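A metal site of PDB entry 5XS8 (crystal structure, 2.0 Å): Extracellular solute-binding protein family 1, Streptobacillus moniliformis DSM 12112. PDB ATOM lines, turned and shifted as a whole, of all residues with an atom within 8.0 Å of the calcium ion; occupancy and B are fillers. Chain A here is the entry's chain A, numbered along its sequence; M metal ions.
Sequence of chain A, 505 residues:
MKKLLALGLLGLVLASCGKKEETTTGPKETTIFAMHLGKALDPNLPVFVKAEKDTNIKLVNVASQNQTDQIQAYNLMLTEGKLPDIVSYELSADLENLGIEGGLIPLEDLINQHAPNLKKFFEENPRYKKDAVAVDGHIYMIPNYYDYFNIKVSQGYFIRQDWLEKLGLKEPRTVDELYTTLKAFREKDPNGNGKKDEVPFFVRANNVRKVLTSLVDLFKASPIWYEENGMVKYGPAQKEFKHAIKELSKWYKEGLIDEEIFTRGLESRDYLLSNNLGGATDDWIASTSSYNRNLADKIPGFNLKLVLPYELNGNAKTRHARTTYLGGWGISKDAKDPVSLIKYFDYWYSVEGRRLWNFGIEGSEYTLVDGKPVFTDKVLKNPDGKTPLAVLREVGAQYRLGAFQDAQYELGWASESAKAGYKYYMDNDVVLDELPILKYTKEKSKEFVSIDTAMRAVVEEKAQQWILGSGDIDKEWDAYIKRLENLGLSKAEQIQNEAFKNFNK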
ATOM      1  N   TRP A 163     -17.432   7.398  10.316  1.00  0.00           N
ATOM      2  CA  TRP A 163     -16.602   7.154   9.142  1.00  0.00           C
ATOM      3  C   TRP A 163     -17.403   7.316   7.875  1.00  0.00           C
ATOM      4  O   TRP A 163     -16.883   7.757   6.833  1.00  0.00           O
ATOM      5  CB  TRP A 163     -15.980   5.762   9.168  1.00  0.00           C
ATOM      6  CG  TRP A 163     -14.915   5.576  10.198  1.00  0.00           C
ATOM      7  CD1 TRP A 163     -14.524   6.507  11.154  1.00  0.00           C
ATOM      8  CD2 TRP A 163     -14.081   4.420  10.382  1.00  0.00           C
ATOM      9  NE1 TRP A 163     -13.508   5.984  11.929  1.00  0.00           N
ATOM     10  CE2 TRP A 163     -13.223   4.698  11.485  1.00  0.00           C
ATOM     11  CE3 TRP A 163     -13.998   3.171   9.753  1.00  0.00           C
ATOM     12  CZ2 TRP A 163     -12.265   3.796  11.930  1.00  0.00           C
ATOM     13  CZ3 TRP A 163     -13.077   2.269  10.219  1.00  0.00           C
ATOM     14  CH2 TRP A 163     -12.194   2.586  11.265  1.00  0.00           C
ATOM     15  N   PHE A 185     -13.648   1.945   3.585  1.00  0.00           N
ATOM     16  CA  PHE A 185     -13.024   1.937   4.909  1.00  0.00           C
ATOM     17  C   PHE A 185     -11.592   1.432   4.837  1.00  0.00           C
ATOM     18  O   PHE A 185     -10.733   1.878   5.607  1.00  0.00           O
ATOM     19  CB  PHE A 185     -13.805   1.080   5.912  1.00  0.00           C
ATOM     20  CG  PHE A 185     -15.131   1.700   6.403  1.00  0.00           C
ATOM     21  CD1 PHE A 185     -15.516   2.954   6.020  1.00  0.00           C
ATOM     22  CD2 PHE A 185     -15.941   0.996   7.293  1.00  0.00           C
ATOM     23  CE1 PHE A 185     -16.722   3.523   6.451  1.00  0.00           C
ATOM     24  CE2 PHE A 185     -17.126   1.561   7.790  1.00  0.00           C
ATOM     25  CZ  PHE A 185     -17.541   2.840   7.339  1.00  0.00           C
ATOM     26  N   ARG A 186     -11.318   0.452   3.981  1.00  0.00           N
ATOM     27  CA  ARG A 186      -9.963  -0.086   3.944  1.00  0.00           C
ATOM     28  C   ARG A 186      -9.004   0.908   3.271  1.00  0.00           C
ATOM     29  O   ARG A 186      -7.862   1.070   3.698  1.00  0.00           O
ATOM     30  CB  ARG A 186      -9.924  -1.422   3.193  1.00  0.00           C
ATOM     31  CG  ARG A 186      -8.550  -2.055   3.063  1.00  0.00           C
ATOM     32  CD  ARG A 186      -7.891  -2.270   4.409  1.00  0.00           C
ATOM     33  NE  ARG A 186      -6.621  -3.043   4.325  1.00  0.00           N
ATOM     34  CZ  ARG A 186      -5.760  -3.181   5.338  1.00  0.00           C
ATOM     35  NH1 ARG A 186      -5.987  -2.605   6.542  1.00  0.00           N
ATOM     36  NH2 ARG A 186      -4.646  -3.884   5.165  1.00  0.00           N
ATOM     37  N   GLU A 187      -9.472   1.567   2.201  1.00  0.00           N
ATOM     38  CA  GLU A 187      -8.549   2.285   1.338  1.00  0.00           C
ATOM     39  C   GLU A 187      -8.381   3.731   1.763  1.00  0.00           C
ATOM     40  O   GLU A 187      -7.304   4.317   1.548  1.00  0.00           O
ATOM     41  CB  GLU A 187      -8.995   2.204  -0.146  1.00  0.00           C
ATOM     42  CG  GLU A 187      -9.173   0.721  -0.746  1.00  0.00           C
ATOM     43  CD  GLU A 187      -7.898  -0.176  -0.704  1.00  0.00           C
ATOM     44  OE1 GLU A 187      -6.822   0.300  -0.255  1.00  0.00           O
ATOM     45  OE2 GLU A 187      -7.946  -1.365  -1.150  1.00  0.00           O
ATOM     46  N   LYS A 188      -9.372   4.328   2.430  1.00  0.00           N
ATOM     47  CA  LYS A 188      -9.447   5.777   2.524  1.00  0.00           C
ATOM     48  C   LYS A 188      -9.172   6.312   3.942  1.00  0.00           C
ATOM     49  O   LYS A 188      -9.637   7.418   4.285  1.00  0.00           O
ATOM     50  CB  LYS A 188     -10.780   6.199   1.937  1.00  0.00           C
ATOM     51  CG  LYS A 188     -10.848   6.026   0.378  1.00  0.00           C
ATOM     52  CD  LYS A 188     -12.216   6.467  -0.112  1.00  0.00           C
ATOM     53  CE  LYS A 188     -12.298   8.020  -0.380  1.00  0.00           C
ATOM     54  NZ  LYS A 188     -11.069   8.589  -1.043  1.00  0.00           N
ATOM     55  N   ASP A 189      -8.500   5.545   4.785  1.00  0.00           N
ATOM     56  CA  ASP A 189      -7.979   6.021   6.052  1.00  0.00           C
ATOM     57  C   ASP A 189      -9.003   6.835   6.889  1.00  0.00           C
ATOM     58  O   ASP A 189      -8.713   7.955   7.290  1.00  0.00           O
ATOM     59  CB  ASP A 189      -6.727   6.849   5.743  1.00  0.00           C
ATOM     60  CG  ASP A 189      -5.980   7.348   7.020  1.00  0.00           C
ATOM     61  OD1 ASP A 189      -5.966   6.617   8.035  1.00  0.00           O
ATOM     62  OD2 ASP A 189      -5.346   8.459   7.009  1.00  0.00           O
ATOM     63  N   PRO A 190     -10.180   6.269   7.127  1.00  0.00           N
ATOM     64  CA  PRO A 190     -11.158   7.056   7.901  1.00  0.00           C
ATOM     65  C   PRO A 190     -10.707   7.368   9.305  1.00  0.00           C
ATOM     66  O   PRO A 190     -11.264   8.299   9.875  1.00  0.00           O
ATOM     67  CB  PRO A 190     -12.418   6.170   7.909  1.00  0.00           C
ATOM     68  CG  PRO A 190     -11.856   4.670   7.672  1.00  0.00           C
ATOM     69  CD  PRO A 190     -10.763   4.992   6.641  1.00  0.00           C
ATOM     70  N   ASN A 191      -9.744   6.626   9.886  1.00  0.00           N
ATOM     71  CA  ASN A 191      -9.319   7.060  11.213  1.00  0.00           C
ATOM     72  C   ASN A 191      -8.258   8.154  11.166  1.00  0.00           C
ATOM     73  O   ASN A 191      -7.802   8.578  12.246  1.00  0.00           O
ATOM     74  CB  ASN A 191      -8.850   5.903  12.134  1.00  0.00           C
ATOM     75  CG  ASN A 191      -7.582   5.214  11.670  1.00  0.00           C
ATOM     76  OD1 ASN A 191      -6.793   5.688  10.831  1.00  0.00           O
ATOM     77  ND2 ASN A 191      -7.365   4.023  12.243  1.00  0.00           N
ATOM     78  N   GLY A 192      -7.960   8.665   9.960  1.00  0.00           N
ATOM     79  CA  GLY A 192      -7.163   9.859   9.746  1.00  0.00           C
ATOM     80  C   GLY A 192      -5.735   9.813  10.251  1.00  0.00           C
ATOM     81  O   GLY A 192      -5.214  10.841  10.660  1.00  0.00           O
ATOM     82  N   ASN A 193      -5.083   8.657  10.242  1.00  0.00           N
ATOM     83  CA  ASN A 193      -3.716   8.646  10.753  1.00  0.00           C
ATOM     84  C   ASN A 193      -2.677   8.423   9.661  1.00  0.00           C
ATOM     85  O   ASN A 193      -1.505   8.186   9.987  1.00  0.00           O
ATOM     86  CB  ASN A 193      -3.573   7.610  11.915  1.00  0.00           C
ATOM     87  CG  ASN A 193      -3.799   6.190  11.487  1.00  0.00           C
ATOM     88  OD1 ASN A 193      -3.976   5.899  10.312  1.00  0.00           O
ATOM     89  ND2 ASN A 193      -3.726   5.281  12.436  1.00  0.00           N
ATOM     90  N   GLY A 194      -3.062   8.491   8.385  1.00  0.00           N
ATOM     91  CA  GLY A 194      -2.171   8.239   7.290  1.00  0.00           C
ATOM     92  C   GLY A 194      -1.645   6.813   7.176  1.00  0.00           C
ATOM     93  O   GLY A 194      -0.719   6.570   6.402  1.00  0.00           O
ATOM     94  N   LYS A 195      -2.204   5.858   7.925  1.00  0.00           N
ATOM     95  CA  LYS A 195      -1.764   4.462   7.859  1.00  0.00           C
ATOM     96  C   LYS A 195      -2.916   3.616   7.321  1.00  0.00           C
ATOM     97  O   LYS A 195      -4.099   3.956   7.509  1.00  0.00           O
ATOM     98  CB  LYS A 195      -1.405   3.937   9.253  1.00  0.00           C
ATOM     99  CG  LYS A 195      -0.308   4.696  10.082  1.00  0.00           C
ATOM    100  CD  LYS A 195      -0.260   3.998  11.445  1.00  0.00           C
ATOM    101  CE  LYS A 195       0.832   4.468  12.429  1.00  0.00           C
ATOM    102  NZ  LYS A 195       0.585   3.839  13.756  1.00  0.00           N
ATOM    103  N   LYS A 196      -2.590   2.527   6.631  1.00  0.00           N
ATOM    104  CA  LYS A 196      -3.609   1.633   6.101  1.00  0.00           C
ATOM    105  C   LYS A 196      -3.828   0.537   7.125  1.00  0.00           C
ATOM    106  O   LYS A 196      -3.442  -0.612   6.944  1.00  0.00           O
ATOM    107  CB  LYS A 196      -3.189   1.091   4.735  1.00  0.00           C
ATOM    108  CG  LYS A 196      -4.329   0.532   3.941  1.00  0.00           C
ATOM    109  CD  LYS A 196      -3.936   0.033   2.584  1.00  0.00           C
ATOM    110  CE  LYS A 196      -4.983  -0.982   2.049  1.00  0.00           C
ATOM    111  NZ  LYS A 196      -4.785  -1.364   0.604  1.00  0.00           N
ATOM    112  N   ASP A 197      -4.386   0.912   8.248  1.00  0.00           N
ATOM    113  CA  ASP A 197      -4.558   0.009   9.394  1.00  0.00           C
ATOM    114  C   ASP A 197      -6.004  -0.381   9.671  1.00  0.00           C
ATOM    115  O   ASP A 197      -6.264  -1.159  10.603  1.00  0.00           O
ATOM    116  CB  ASP A 197      -3.997   0.630  10.686  1.00  0.00           C
ATOM    117  CG  ASP A 197      -4.592   2.034  10.996  1.00  0.00           C
ATOM    118  OD1 ASP A 197      -5.204   2.691  10.130  1.00  0.00           O
ATOM    119  OD2 ASP A 197      -4.438   2.501  12.143  1.00  0.00           O
ATOM    120  N   GLU A 198      -6.957   0.217   8.950  1.00  0.00           N
ATOM    121  CA  GLU A 198      -8.371  -0.027   9.194  1.00  0.00           C
ATOM    122  C   GLU A 198      -8.726  -1.512   9.001  1.00  0.00           C
ATOM    123  O   GLU A 198      -8.248  -2.195   8.084  1.00  0.00           O
ATOM    124  CB  GLU A 198      -9.227   0.816   8.224  1.00  0.00           C
ATOM    125  CG  GLU A 198      -9.436   2.306   8.671  1.00  0.00           C
ATOM    126  CD  GLU A 198      -8.205   3.198   8.382  1.00  0.00           C
ATOM    127  OE1 GLU A 198      -7.216   2.709   7.767  1.00  0.00           O
ATOM    128  OE2 GLU A 198      -8.239   4.389   8.812  1.00  0.00           O
ATOM    129  N   VAL A 199      -9.588  -1.983   9.869  1.00  0.00           N
ATOM    130  CA  VAL A 199     -10.168  -3.312   9.834  1.00  0.00           C
ATOM    131  C   VAL A 199     -11.667  -3.122   9.590  1.00  0.00           C
ATOM    132  O   VAL A 199     -12.414  -2.830  10.524  1.00  0.00           O
ATOM    133  CB  VAL A 199      -9.884  -4.026  11.156  1.00  0.00           C
ATOM    134  CG1 VAL A 199     -10.450  -5.467  11.163  1.00  0.00           C
ATOM    135  CG2 VAL A 199      -8.345  -4.038  11.411  1.00  0.00           C
ATOM    136  N   ASN A 276      -9.594   2.404  17.502  1.00  0.00           N
ATOM    137  CA  ASN A 276     -10.105   3.080  16.325  1.00  0.00           C
ATOM    138  C   ASN A 276      -9.763   2.379  15.025  1.00  0.00           C
ATOM    139  O   ASN A 276      -9.495   3.026  14.035  1.00  0.00           O
ATOM    140  CB  ASN A 276      -9.630   4.549  16.271  1.00  0.00           C
ATOM    141  CG  ASN A 276     -10.594   5.446  15.499  1.00  0.00           C
ATOM    142  OD1 ASN A 276     -11.744   5.057  15.190  1.00  0.00           O
ATOM    143  ND2 ASN A 276     -10.149   6.621  15.149  1.00  0.00           N
ATOM    144  N   LEU A 277      -9.718   1.046  15.020  1.00  0.00           N
ATOM    145  CA  LEU A 277      -9.484   0.269  13.802  1.00  0.00           C
ATOM    146  C   LEU A 277     -10.748  -0.320  13.165  1.00  0.00           C
ATOM    147  O   LEU A 277     -10.773  -0.495  11.939  1.00  0.00           O
ATOM    148  CB  LEU A 277      -8.515  -0.893  14.097  1.00  0.00           C
ATOM    149  CG  LEU A 277      -7.254  -0.390  14.774  1.00  0.00           C
ATOM    150  CD1 LEU A 277      -6.486  -1.645  15.174  1.00  0.00           C
ATOM    151  CD2 LEU A 277      -6.490   0.435  13.684  1.00  0.00           C
HETATM  152 CA    CA M   1      -5.823   4.664   9.108  1.00  0.00          CA
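O of Glu 198 is in hydrogen-bond range of NH1 of Arg 186.
ND2 of Asn 191 is in hydrogen-bond range of O of Asn 276, at 3.0 Å.
The backbone NH (N) of Gly 194 sits at hydrogen-bond distance from the side-chain carboxylate (OD2) of Asp 189, at 2.7 Å.
The side-chain carboxylate (OD1) of Asp 189 sits close to the backbone NH (N) of Gly 192, 3.4 Å away.
The nearest printed residue that does not touch the calcium ion is Lys 196 (4.6 Å).
The calcium ion is bound by OD1 of Asn 191 (2.2 Å).
OD1 of Asp 189 is bound to the calcium ion.
OD1 of Asp 197 binds the calcium ion (2.3 Å).
The calcium ion is bound by OE2 of Glu 198, at 2.4 Å.
O of Lys 195 binds the calcium ion.
The calcium ion is bound by the side-chain amide oxygen (OD1) of Asn 193, at 2.5 Å.
OE1 of Glu 198 binds the calcium ion.
The calcium ion has seven donor atoms within binding distance.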
